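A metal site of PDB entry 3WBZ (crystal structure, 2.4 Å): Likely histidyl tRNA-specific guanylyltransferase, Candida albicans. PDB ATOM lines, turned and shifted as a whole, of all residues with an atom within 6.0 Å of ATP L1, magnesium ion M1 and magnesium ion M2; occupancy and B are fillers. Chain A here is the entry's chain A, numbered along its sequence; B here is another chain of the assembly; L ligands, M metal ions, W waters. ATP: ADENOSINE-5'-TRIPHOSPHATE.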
ATOM      1  N   ASP A  32      23.487 -23.235 -12.041  1.00  0.00           N
ATOM      2  CA  ASP A  32      24.051 -24.154 -11.045  1.00  0.00           C
ATOM      3  C   ASP A  32      25.380 -23.622 -10.542  1.00  0.00           C
ATOM      4  O   ASP A  32      26.256 -23.252 -11.336  1.00  0.00           O
ATOM      5  CB  ASP A  32      24.234 -25.552 -11.650  1.00  0.00           C
ATOM      6  CG  ASP A  32      24.818 -26.538 -10.647  1.00  0.00           C
ATOM      7  OD1 ASP A  32      26.020 -26.449 -10.374  1.00  0.00           O
ATOM      8  OD2 ASP A  32      24.088 -27.415 -10.148  1.00  0.00           O
ATOM      9  N   GLY A  33      25.557 -23.634  -9.224  1.00  0.00           N
ATOM     10  CA  GLY A  33      26.748 -23.090  -8.603  1.00  0.00           C
ATOM     11  C   GLY A  33      28.004 -23.783  -9.079  1.00  0.00           C
ATOM     12  O   GLY A  33      28.087 -25.003  -9.113  1.00  0.00           O
ATOM     13  N   LYS A  34      29.011 -23.000  -9.432  1.00  0.00           N
ATOM     14  CA  LYS A  34      30.283 -23.545  -9.890  1.00  0.00           C
ATOM     15  C   LYS A  34      31.180 -23.961  -8.709  1.00  0.00           C
ATOM     16  O   LYS A  34      31.523 -23.131  -7.854  1.00  0.00           O
ATOM     17  CB  LYS A  34      31.015 -22.519 -10.758  1.00  0.00           C
ATOM     18  CG  LYS A  34      32.395 -22.992 -11.235  1.00  0.00           C
ATOM     19  CD  LYS A  34      33.227 -21.836 -11.774  1.00  0.00           C
ATOM     20  CE  LYS A  34      34.665 -22.286 -11.964  1.00  0.00           C
ATOM     21  NZ  LYS A  34      34.712 -23.586 -12.753  1.00  0.00           N
ATOM     22  N   GLY A  35      31.540 -25.242  -8.679  1.00  0.00           N
ATOM     23  CA  GLY A  35      32.405 -25.761  -7.622  1.00  0.00           C
ATOM     24  C   GLY A  35      31.821 -25.566  -6.234  1.00  0.00           C
ATOM     25  O   GLY A  35      32.527 -25.196  -5.295  1.00  0.00           O
ATOM     26  N   PHE A  36      30.536 -25.828  -6.068  1.00  0.00           N
ATOM     27  CA  PHE A  36      29.935 -25.631  -4.762  1.00  0.00           C
ATOM     28  C   PHE A  36      30.217 -26.746  -3.778  1.00  0.00           C
ATOM     29  O   PHE A  36      29.922 -26.603  -2.586  1.00  0.00           O
ATOM     30  CB  PHE A  36      28.437 -25.440  -4.880  1.00  0.00           C
ATOM     31  CG  PHE A  36      28.012 -24.004  -4.769  1.00  0.00           C
ATOM     32  CD1 PHE A  36      28.502 -23.062  -5.666  1.00  0.00           C
ATOM     33  CD2 PHE A  36      27.133 -23.584  -3.762  1.00  0.00           C
ATOM     34  CE1 PHE A  36      28.091 -21.721  -5.590  1.00  0.00           C
ATOM     35  CE2 PHE A  36      26.722 -22.244  -3.686  1.00  0.00           C
ATOM     36  CZ  PHE A  36      27.212 -21.314  -4.598  1.00  0.00           C
ATOM     37  N   HIS A  37      30.794 -27.865  -4.227  1.00  0.00           N
ATOM     38  CA  HIS A  37      31.296 -28.814  -3.246  1.00  0.00           C
ATOM     39  C   HIS A  37      32.438 -28.130  -2.458  1.00  0.00           C
ATOM     40  O   HIS A  37      32.418 -28.115  -1.223  1.00  0.00           O
ATOM     41  CB  HIS A  37      31.769 -30.124  -3.877  1.00  0.00           C
ATOM     42  CG  HIS A  37      32.260 -31.113  -2.875  1.00  0.00           C
ATOM     43  ND1 HIS A  37      31.405 -31.913  -2.142  1.00  0.00           N
ATOM     44  CD2 HIS A  37      33.500 -31.366  -2.394  1.00  0.00           C
ATOM     45  CE1 HIS A  37      32.103 -32.650  -1.300  1.00  0.00           C
ATOM     46  NE2 HIS A  37      33.377 -32.327  -1.427  1.00  0.00           N
ATOM     47  N   LYS A  38      33.444 -27.573  -3.144  1.00  0.00           N
ATOM     48  CA  LYS A  38      34.514 -26.841  -2.455  1.00  0.00           C
ATOM     49  C   LYS A  38      34.032 -25.624  -1.703  1.00  0.00           C
ATOM     50  O   LYS A  38      34.469 -25.353  -0.581  1.00  0.00           O
ATOM     51  CB  LYS A  38      35.631 -26.359  -3.391  1.00  0.00           C
ATOM     52  CG  LYS A  38      36.599 -27.418  -3.889  1.00  0.00           C
ATOM     53  CD  LYS A  38      37.668 -26.772  -4.771  1.00  0.00           C
ATOM     54  CE  LYS A  38      38.629 -27.794  -5.356  1.00  0.00           C
ATOM     55  NZ  LYS A  38      39.663 -27.152  -6.249  1.00  0.00           N
ATOM     56  N   SER A  40      31.165 -25.147  -0.330  1.00  0.00           N
ATOM     57  CA  SER A  40      30.487 -25.567   0.887  1.00  0.00           C
ATOM     58  C   SER A  40      31.459 -26.092   1.954  1.00  0.00           C
ATOM     59  O   SER A  40      31.173 -26.055   3.133  1.00  0.00           O
ATOM     60  CB  SER A  40      29.422 -26.621   0.572  1.00  0.00           C
ATOM     61  OG  SER A  40      30.023 -27.833   0.165  1.00  0.00           O
ATOM     62  N   PHE A  45      29.669 -25.343   5.428  1.00  0.00           N
ATOM     63  CA  PHE A  45      28.236 -25.620   5.403  1.00  0.00           C
ATOM     64  C   PHE A  45      27.916 -26.776   6.346  1.00  0.00           C
ATOM     65  O   PHE A  45      28.670 -27.735   6.443  1.00  0.00           O
ATOM     66  CB  PHE A  45      27.756 -26.007   3.983  1.00  0.00           C
ATOM     67  CG  PHE A  45      27.628 -24.853   3.023  1.00  0.00           C
ATOM     68  CD1 PHE A  45      28.299 -23.660   3.216  1.00  0.00           C
ATOM     69  CD2 PHE A  45      26.786 -24.954   1.924  1.00  0.00           C
ATOM     70  CE1 PHE A  45      28.175 -22.609   2.320  1.00  0.00           C
ATOM     71  CE2 PHE A  45      26.647 -23.901   1.012  1.00  0.00           C
ATOM     72  CZ  PHE A  45      27.356 -22.720   1.217  1.00  0.00           C
ATOM     73  N   GLU A  46      26.785 -26.715   7.020  1.00  0.00           N
ATOM     74  CA  GLU A  46      26.281 -27.896   7.713  1.00  0.00           C
ATOM     75  C   GLU A  46      25.961 -28.991   6.691  1.00  0.00           C
ATOM     76  O   GLU A  46      25.564 -28.741   5.555  1.00  0.00           O
ATOM     77  CB  GLU A  46      25.024 -27.559   8.513  1.00  0.00           C
ATOM     78  CG  GLU A  46      25.263 -26.562   9.617  1.00  0.00           C
ATOM     79  CD  GLU A  46      24.064 -26.430  10.532  1.00  0.00           C
ATOM     80  OE1 GLU A  46      23.155 -27.296  10.443  1.00  0.00           O
ATOM     81  OE2 GLU A  46      24.044 -25.441  11.328  1.00  0.00           O
ATOM     82  N   LYS A  47      26.134 -30.222   7.149  1.00  0.00           N
ATOM     83  CA  LYS A  47      25.861 -31.374   6.325  1.00  0.00           C
ATOM     84  C   LYS A  47      24.802 -32.200   7.045  1.00  0.00           C
ATOM     85  O   LYS A  47      24.788 -32.256   8.263  1.00  0.00           O
ATOM     86  CB  LYS A  47      27.156 -32.155   6.100  1.00  0.00           C
ATOM     87  CG  LYS A  47      28.188 -31.354   5.334  1.00  0.00           C
ATOM     88  CD  LYS A  47      27.686 -31.086   3.899  1.00  0.00           C
ATOM     89  CE  LYS A  47      28.696 -30.304   3.082  1.00  0.00           C
ATOM     90  NZ  LYS A  47      28.402 -30.392   1.633  1.00  0.00           N
ATOM     91  N   PRO A  48      23.898 -32.837   6.279  1.00  0.00           N
ATOM     92  CA  PRO A  48      23.830 -32.848   4.812  1.00  0.00           C
ATOM     93  C   PRO A  48      23.305 -31.535   4.216  1.00  0.00           C
ATOM     94  O   PRO A  48      23.703 -31.193   3.109  1.00  0.00           O
ATOM     95  CB  PRO A  48      22.882 -34.002   4.508  1.00  0.00           C
ATOM     96  CG  PRO A  48      21.981 -34.067   5.739  1.00  0.00           C
ATOM     97  CD  PRO A  48      22.859 -33.707   6.892  1.00  0.00           C
ATOM     98  N   ASN A  49      22.420 -30.855   4.917  1.00  0.00           N
ATOM     99  CA  ASN A  49      21.838 -29.609   4.391  1.00  0.00           C
ATOM    100  C   ASN A  49      22.080 -28.407   5.276  1.00  0.00           C
ATOM    101  O   ASN A  49      21.864 -28.436   6.489  1.00  0.00           O
ATOM    102  CB  ASN A  49      20.332 -29.772   4.183  1.00  0.00           C
ATOM    103  CG  ASN A  49      20.004 -30.908   3.224  1.00  0.00           C
ATOM    104  OD1 ASN A  49      20.309 -30.833   2.041  1.00  0.00           O
ATOM    105  ND2 ASN A  49      19.330 -31.943   3.729  1.00  0.00           N
ATOM    106  N   ASP A  50      22.546 -27.327   4.657  1.00  0.00           N
ATOM    107  CA  ASP A  50      22.700 -26.080   5.380  1.00  0.00           C
ATOM    108  C   ASP A  50      21.492 -25.210   5.092  1.00  0.00           C
ATOM    109  O   ASP A  50      21.309 -24.724   3.970  1.00  0.00           O
ATOM    110  CB  ASP A  50      23.988 -25.370   4.982  1.00  0.00           C
ATOM    111  CG  ASP A  50      24.345 -24.244   5.925  1.00  0.00           C
ATOM    112  OD1 ASP A  50      23.611 -23.231   5.942  1.00  0.00           O
ATOM    113  OD2 ASP A  50      25.360 -24.354   6.631  1.00  0.00           O
ATOM    114  N   LEU A  51      20.668 -25.017   6.101  1.00  0.00           N
ATOM    115  CA  LEU A  51      19.408 -24.312   5.955  1.00  0.00           C
ATOM    116  C   LEU A  51      19.594 -22.883   5.471  1.00  0.00           C
ATOM    117  O   LEU A  51      18.940 -22.464   4.509  1.00  0.00           O
ATOM    118  CB  LEU A  51      18.642 -24.334   7.272  1.00  0.00           C
ATOM    119  CG  LEU A  51      17.422 -23.418   7.329  1.00  0.00           C
ATOM    120  CD1 LEU A  51      16.388 -23.815   6.295  1.00  0.00           C
ATOM    121  CD2 LEU A  51      16.794 -23.449   8.713  1.00  0.00           C
ATOM    122  N   ALA A  53      22.090 -21.591   3.947  1.00  0.00           N
ATOM    123  CA  ALA A  53      22.646 -21.614   2.608  1.00  0.00           C
ATOM    124  C   ALA A  53      21.527 -21.769   1.571  1.00  0.00           C
ATOM    125  O   ALA A  53      21.570 -21.145   0.523  1.00  0.00           O
ATOM    126  CB  ALA A  53      23.674 -22.718   2.482  1.00  0.00           C
ATOM    127  N   LEU A  54      20.537 -22.603   1.863  1.00  0.00           N
ATOM    128  CA  LEU A  54      19.374 -22.739   0.994  1.00  0.00           C
ATOM    129  C   LEU A  54      18.499 -21.481   1.017  1.00  0.00           C
ATOM    130  O   LEU A  54      17.883 -21.110   0.006  1.00  0.00           O
ATOM    131  CB  LEU A  54      18.549 -23.969   1.372  1.00  0.00           C
ATOM    132  CG  LEU A  54      19.206 -25.315   1.019  1.00  0.00           C
ATOM    133  CD1 LEU A  54      18.411 -26.468   1.610  1.00  0.00           C
ATOM    134  CD2 LEU A  54      19.286 -25.486  -0.489  1.00  0.00           C
ATOM    135  N   ASP A  77      16.951 -26.587  -5.700  1.00  0.00           N
ATOM    136  CA  ASP A  77      17.426 -27.434  -4.610  1.00  0.00           C
ATOM    137  C   ASP A  77      18.949 -27.498  -4.695  1.00  0.00           C
ATOM    138  O   ASP A  77      19.514 -27.267  -5.778  1.00  0.00           O
ATOM    139  CB  ASP A  77      16.832 -28.827  -4.717  1.00  0.00           C
ATOM    140  CG  ASP A  77      17.465 -29.633  -5.796  1.00  0.00           C
ATOM    141  OD1 ASP A  77      17.108 -29.371  -6.968  1.00  0.00           O
ATOM    142  OD2 ASP A  77      18.285 -30.531  -5.499  1.00  0.00           O
ATOM    143  N   SER A  78      19.612 -27.802  -3.581  1.00  0.00           N
ATOM    144  CA  SER A  78      21.066 -27.858  -3.582  1.00  0.00           C
ATOM    145  C   SER A  78      21.628 -26.526  -4.099  1.00  0.00           C
ATOM    146  O   SER A  78      21.256 -25.460  -3.610  1.00  0.00           O
ATOM    147  CB  SER A  78      21.563 -29.041  -4.416  1.00  0.00           C
ATOM    148  OG  SER A  78      22.983 -29.102  -4.388  1.00  0.00           O
ATOM    149  N   ASP A  79      22.527 -26.582  -5.092  1.00  0.00           N
ATOM    150  CA  ASP A  79      23.088 -25.340  -5.637  1.00  0.00           C
ATOM    151  C   ASP A  79      22.484 -24.928  -6.989  1.00  0.00           C
ATOM    152  O   ASP A  79      23.134 -24.219  -7.756  1.00  0.00           O
ATOM    153  CB  ASP A  79      24.607 -25.470  -5.784  1.00  0.00           C
ATOM    154  CG  ASP A  79      25.010 -26.427  -6.898  1.00  0.00           C
ATOM    155  OD1 ASP A  79      24.179 -27.299  -7.219  1.00  0.00           O
ATOM    156  OD2 ASP A  79      26.144 -26.300  -7.444  1.00  0.00           O
ATOM    157  N   GLU A  80      21.253 -25.356  -7.300  1.00  0.00           N
ATOM    158  CA  GLU A  80      20.662 -25.078  -8.615  1.00  0.00           C
ATOM    159  C   GLU A  80      19.281 -24.429  -8.517  1.00  0.00           C
ATOM    160  O   GLU A  80      18.565 -24.603  -7.543  1.00  0.00           O
ATOM    161  CB  GLU A  80      20.579 -26.373  -9.466  1.00  0.00           C
ATOM    162  CG  GLU A  80      19.280 -27.152  -9.327  1.00  0.00           C
ATOM    163  CD  GLU A  80      19.216 -28.423 -10.186  1.00  0.00           C
ATOM    164  OE1 GLU A  80      20.237 -29.169 -10.238  1.00  0.00           O
ATOM    165  OE2 GLU A  80      18.122 -28.682 -10.785  1.00  0.00           O
ATOM    166  N   ASN A 163      22.575 -38.147   0.386  1.00  0.00           N
ATOM    167  CA  ASN A 163      23.413 -37.292   1.225  1.00  0.00           C
ATOM    168  C   ASN A 163      23.034 -37.374   2.690  1.00  0.00           C
ATOM    169  O   ASN A 163      23.909 -37.346   3.562  1.00  0.00           O
ATOM    170  CB  ASN A 163      23.334 -35.823   0.790  1.00  0.00           C
ATOM    171  CG  ASN A 163      23.989 -35.586  -0.535  1.00  0.00           C
ATOM    172  OD1 ASN A 163      24.938 -36.276  -0.879  1.00  0.00           O
ATOM    173  ND2 ASN A 163      23.521 -34.578  -1.260  1.00  0.00           N
ATOM    174  N   LYS B  98      29.283 -21.948 -21.323  1.00  0.00           N
ATOM    175  CA  LYS B  98      30.115 -21.949 -20.135  1.00  0.00           C
ATOM    176  C   LYS B  98      31.050 -20.719 -20.044  1.00  0.00           C
ATOM    177  O   LYS B  98      31.185 -20.109 -18.991  1.00  0.00           O
ATOM    178  CB  LYS B  98      30.945 -23.226 -20.077  1.00  0.00           C
ATOM    179  CG  LYS B  98      30.142 -24.468 -19.727  1.00  0.00           C
ATOM    180  CD  LYS B  98      29.787 -24.500 -18.252  1.00  0.00           C
ATOM    181  CE  LYS B  98      29.140 -25.834 -17.909  1.00  0.00           C
ATOM    182  NZ  LYS B  98      28.814 -25.961 -16.470  1.00  0.00           N
HETATM  183  PG  ATP L   1      29.912 -28.082 -10.737  1.00  0.00           P
HETATM  184  O1G ATP L   1      30.044 -29.214 -11.723  1.00  0.00           O
HETATM  185  O2G ATP L   1      28.481 -27.622 -10.504  1.00  0.00           O
HETATM  186  O3G ATP L   1      30.931 -26.995 -10.971  1.00  0.00           O
HETATM  187  PB  ATP L   1      29.676 -28.671  -7.922  1.00  0.00           P
HETATM  188  O1B ATP L   1      30.764 -28.919  -6.920  1.00  0.00           O
HETATM  189  O2B ATP L   1      28.842 -27.426  -7.779  1.00  0.00           O
HETATM  190  O3B ATP L   1      30.392 -28.784  -9.363  1.00  0.00           O
HETATM  191  PA  ATP L   1      27.136 -30.123  -7.973  1.00  0.00           P
HETATM  192  O1A ATP L   1      26.645 -31.374  -8.612  1.00  0.00           O
HETATM  193  O2A ATP L   1      26.482 -28.821  -8.404  1.00  0.00           O
HETATM  194  O3A ATP L   1      28.751 -30.017  -8.017  1.00  0.00           O
HETATM  195  O5' ATP L   1      26.982 -30.300  -6.390  1.00  0.00           O
HETATM  196  C5' ATP L   1      26.788 -29.221  -5.467  1.00  0.00           C
HETATM  197  C4' ATP L   1      27.349 -29.617  -4.090  1.00  0.00           C
HETATM  198  O4' ATP L   1      27.464 -28.500  -3.188  1.00  0.00           O
HETATM  199  C3' ATP L   1      26.507 -30.649  -3.354  1.00  0.00           C
HETATM  200  O3' ATP L   1      26.908 -31.980  -3.677  1.00  0.00           O
HETATM  201  C2' ATP L   1      26.864 -30.388  -1.922  1.00  0.00           C
HETATM  202  O2' ATP L   1      28.127 -31.044  -1.752  1.00  0.00           O
HETATM  203  C1' ATP L   1      27.173 -28.913  -1.843  1.00  0.00           C
HETATM  204  N9  ATP L   1      26.013 -28.113  -1.377  1.00  0.00           N
HETATM  205  C8  ATP L   1      25.370 -27.242  -2.149  1.00  0.00           C
HETATM  206  N7  ATP L   1      24.384 -26.630  -1.459  1.00  0.00           N
HETATM  207  C5  ATP L   1      24.407 -27.106  -0.207  1.00  0.00           C
HETATM  208  C6  ATP L   1      23.637 -26.868   1.030  1.00  0.00           C
HETATM  209  N6  ATP L   1      22.629 -25.966   1.041  1.00  0.00           N
HETATM  210  N1  ATP L   1      23.985 -27.557   2.124  1.00  0.00           N
HETATM  211  C2  ATP L   1      25.004 -28.416   2.116  1.00  0.00           C
HETATM  212  N3  ATP L   1      25.746 -28.675   1.042  1.00  0.00           N
HETATM  213  C4  ATP L   1      25.494 -28.068  -0.148  1.00  0.00           C
HETATM  214  PG  ATP L   2      27.747 -29.475 -17.586  1.00  0.00           P
HETATM  215  O1G ATP L   2      26.833 -29.169 -18.738  1.00  0.00           O
HETATM  216  O2G ATP L   2      27.433 -28.670 -16.335  1.00  0.00           O
HETATM  217  O3G ATP L   2      29.223 -29.599 -17.926  1.00  0.00           O
HETATM  218  PB  ATP L   2      26.885 -31.666 -15.865  1.00  0.00           P
HETATM  219  O1B ATP L   2      27.118 -33.159 -15.908  1.00  0.00           O
HETATM  220  O2B ATP L   2      27.368 -30.899 -14.657  1.00  0.00           O
HETATM  221  O3B ATP L   2      27.433 -31.049 -17.259  1.00  0.00           O
HETATM  222  PA  ATP L   2      24.249 -30.374 -15.554  1.00  0.00           P
HETATM  223  O1A ATP L   2      23.266 -30.084 -16.694  1.00  0.00           O
HETATM  224  O2A ATP L   2      24.946 -29.188 -14.889  1.00  0.00           O
HETATM  225  O3A ATP L   2      25.284 -31.492 -16.118  1.00  0.00           O
HETATM  226  O5' ATP L   2      23.437 -31.169 -14.413  1.00  0.00           O
HETATM  227  C5' ATP L   2      22.019 -31.244 -14.521  1.00  0.00           C
HETATM  228  C4' ATP L   2      21.543 -32.655 -14.171  1.00  0.00           C
HETATM  229  O4' ATP L   2      21.613 -33.479 -15.334  1.00  0.00           O
HETATM  230  C3' ATP L   2      22.419 -33.307 -13.116  1.00  0.00           C
HETATM  231  O3' ATP L   2      21.559 -33.970 -12.185  1.00  0.00           O
HETATM  232  C2' ATP L   2      23.187 -34.379 -13.850  1.00  0.00           C
HETATM  233  O2' ATP L   2      23.336 -35.468 -12.947  1.00  0.00           O
HETATM  234  C1' ATP L   2      22.277 -34.704 -15.023  1.00  0.00           C
HETATM  235  N9  ATP L   2      22.993 -35.133 -16.254  1.00  0.00           N
HETATM  236  C8  ATP L   2      24.199 -34.704 -16.649  1.00  0.00           C
HETATM  237  N7  ATP L   2      24.560 -35.276 -17.823  1.00  0.00           N
HETATM  238  C5  ATP L   2      23.564 -36.086 -18.203  1.00  0.00           C
HETATM  239  C6  ATP L   2      23.302 -36.990 -19.349  1.00  0.00           C
HETATM  240  N6  ATP L   2      24.222 -37.124 -20.325  1.00  0.00           N
HETATM  241  N1  ATP L   2      22.129 -37.652 -19.374  1.00  0.00           N
HETATM  242  C2  ATP L   2      21.217 -37.523 -18.393  1.00  0.00           C
HETATM  243  N3  ATP L   2      21.387 -36.727 -17.315  1.00  0.00           N
HETATM  244  C4  ATP L   2      22.530 -35.997 -17.165  1.00  0.00           C
HETATM  245 MG    MG M   1      27.346 -26.950  -9.101  1.00  0.00          MG
HETATM  246 MG    MG M   2      24.355 -28.878  -8.622  1.00  0.00          MG
HETATM  247 MG    MG M   3      26.932 -28.741 -14.486  1.00  0.00          MG
HETATM  248  O   HOH W   1      24.071 -30.509  -7.063  1.00  0.00           O
HETATM  249  O   HOH W   2      33.879 -28.316  -6.158  1.00  0.00           O
HETATM  250  O   HOH W   3      21.464 -29.073   0.124  1.00  0.00           O
HETATM  251  O   HOH W   4      26.649 -28.896 -12.515  1.00  0.00           O
HETATM  252  O   HOH W   5      22.721 -24.281  -1.582  1.00  0.00           O
HETATM  253  O   HOH W   6      31.744 -26.522 -13.437  1.00  0.00           O
HETATM  254  O   HOH W   7      28.035 -25.315 -12.389  1.00  0.00           O
HETATM  255  O   HOH W   8      22.178 -29.338  -8.476  1.00  0.00           O
HETATM  256  O   HOH W   9      28.637 -31.449 -12.335  1.00  0.00           O
HETATM  257  O   HOH W  10      24.461 -30.400 -10.091  1.00  0.00           O
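An oxygen (O3G) of ATP L2 is in salt-bridge range of the side-chain amino group (NZ) of Lys 98 of chain B (3.9 Å). O1B of ATP L1 is in hydrogen-bond range of N of Phe 36 (3.2 Å). A ring nitrogen (ND1) of His 37 is in hydrogen-bond range of an oxygen (O2') of ATP L1. N of His 37 is in hydrogen-bond range of O1B of ATP L1 (2.9 Å). An oxygen (O3G) of ATP L1 sits at hydrogen-bond distance from the backbone NH (N) of Gly 35 (2.9 Å). N1 of ATP L1 lies within hydrogen-bond range of N of Asp 50, 2.9 Å away. NZ of Lys 47 is in hydrogen-bond range of N3 of ATP L1 (3.2 Å). A nitrogen (N6) of ATP L1 is in hydrogen-bond range of the backbone carbonyl oxygen of Asp 50 (3.4 Å).
N of Phe 45 is in hydrogen-bond range of O of Ser 40, at 2.8 Å. OG of Ser 40 sits at hydrogen-bond distance from O of Phe 36 (3.0 Å). OG of Ser 40 lies within hydrogen-bond range of O of His 37 (2.8 Å). OD1 of Asp 50 is in hydrogen-bond range of N of Ala 53 (3.0 Å). The backbone NH (N) of Glu 46 is in hydrogen-bond range of the side-chain carboxylate (OD2) of Asp 50, 2.8 Å away. The side-chain hydroxyl (OG) of Ser 40 lies within hydrogen-bond range of the side-chain amino group (NZ) of Lys 47, 3.4 Å away.
Residues that only touch ATP L1: Lys 34, Ser 40, Phe 45, Glu 46, Pro 48, Asn 49, Ala 53, Leu 54 and Ser 78. Hydrophobic or aromatic side chains within 4 Å of ATP L1: Phe 36, His 37, Phe 45, Ala 53 and Leu 54. Within 4 Å of ATP L1: Asp 32, Gly 33, Lys 34, Gly 35, Phe 36, His 37, Ser 40, Phe 45, Glu 46, Lys 47, Pro 48, Asn 49, Asp 50, Ala 53, Leu 54, Ser 78 and Asp 79. Along chain A the residues within 4 Å of ATP L1 span positions 32 to 79. The nearest printed residue that does not touch ATP L1 is Lys 38 (4.8 Å).
Within 4 Å of magnesium ion M1: Asp 32, Gly 33 and Asp 79.
Of the 23 residues printed, 2 come within 4 Å of magnesium ion M2.
The side-chain carboxylate (OD1) of Asp 32 is bound to magnesium ion M1 (1.9 Å). Magnesium ion M1 is bound by an oxygen (O2G) of ATP L1. O2B of ATP L1 binds magnesium ion M1, 2.1 Å away. Magnesium ion M1 is bound by the backbone carbonyl oxygen (O) of Gly 33. OD2 of Asp 79 is bound to magnesium ion M1. O2A of ATP L1 is bound to magnesium ion M1.
Magnesium ion M2 is bound by water W10 (2.1 Å), OD1 of Asp 79 (2.1 Å), OD2 of Asp 32 (2.1 Å), O2A of ATP L1 (2.1 Å), water W8 (2.2 Å) and water W1 (2.3 Å).
Water W1 lies within hydrogen-bond range of O5' of ATP L1 (3.0 Å) and OG of Ser 78 (3.2 Å). Water W5 bridges O of Ser 78 (2.8 Å) and N7 of ATP L1 (2.9 Å). Water W3 bridges OD1 of Asn 49 (2.8 Å) and N6 of ATP L1 (3.4 Å). Water W2 bridges N of Lys 38 (3.1 Å) and O1B of ATP L1 (3.3 Å).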
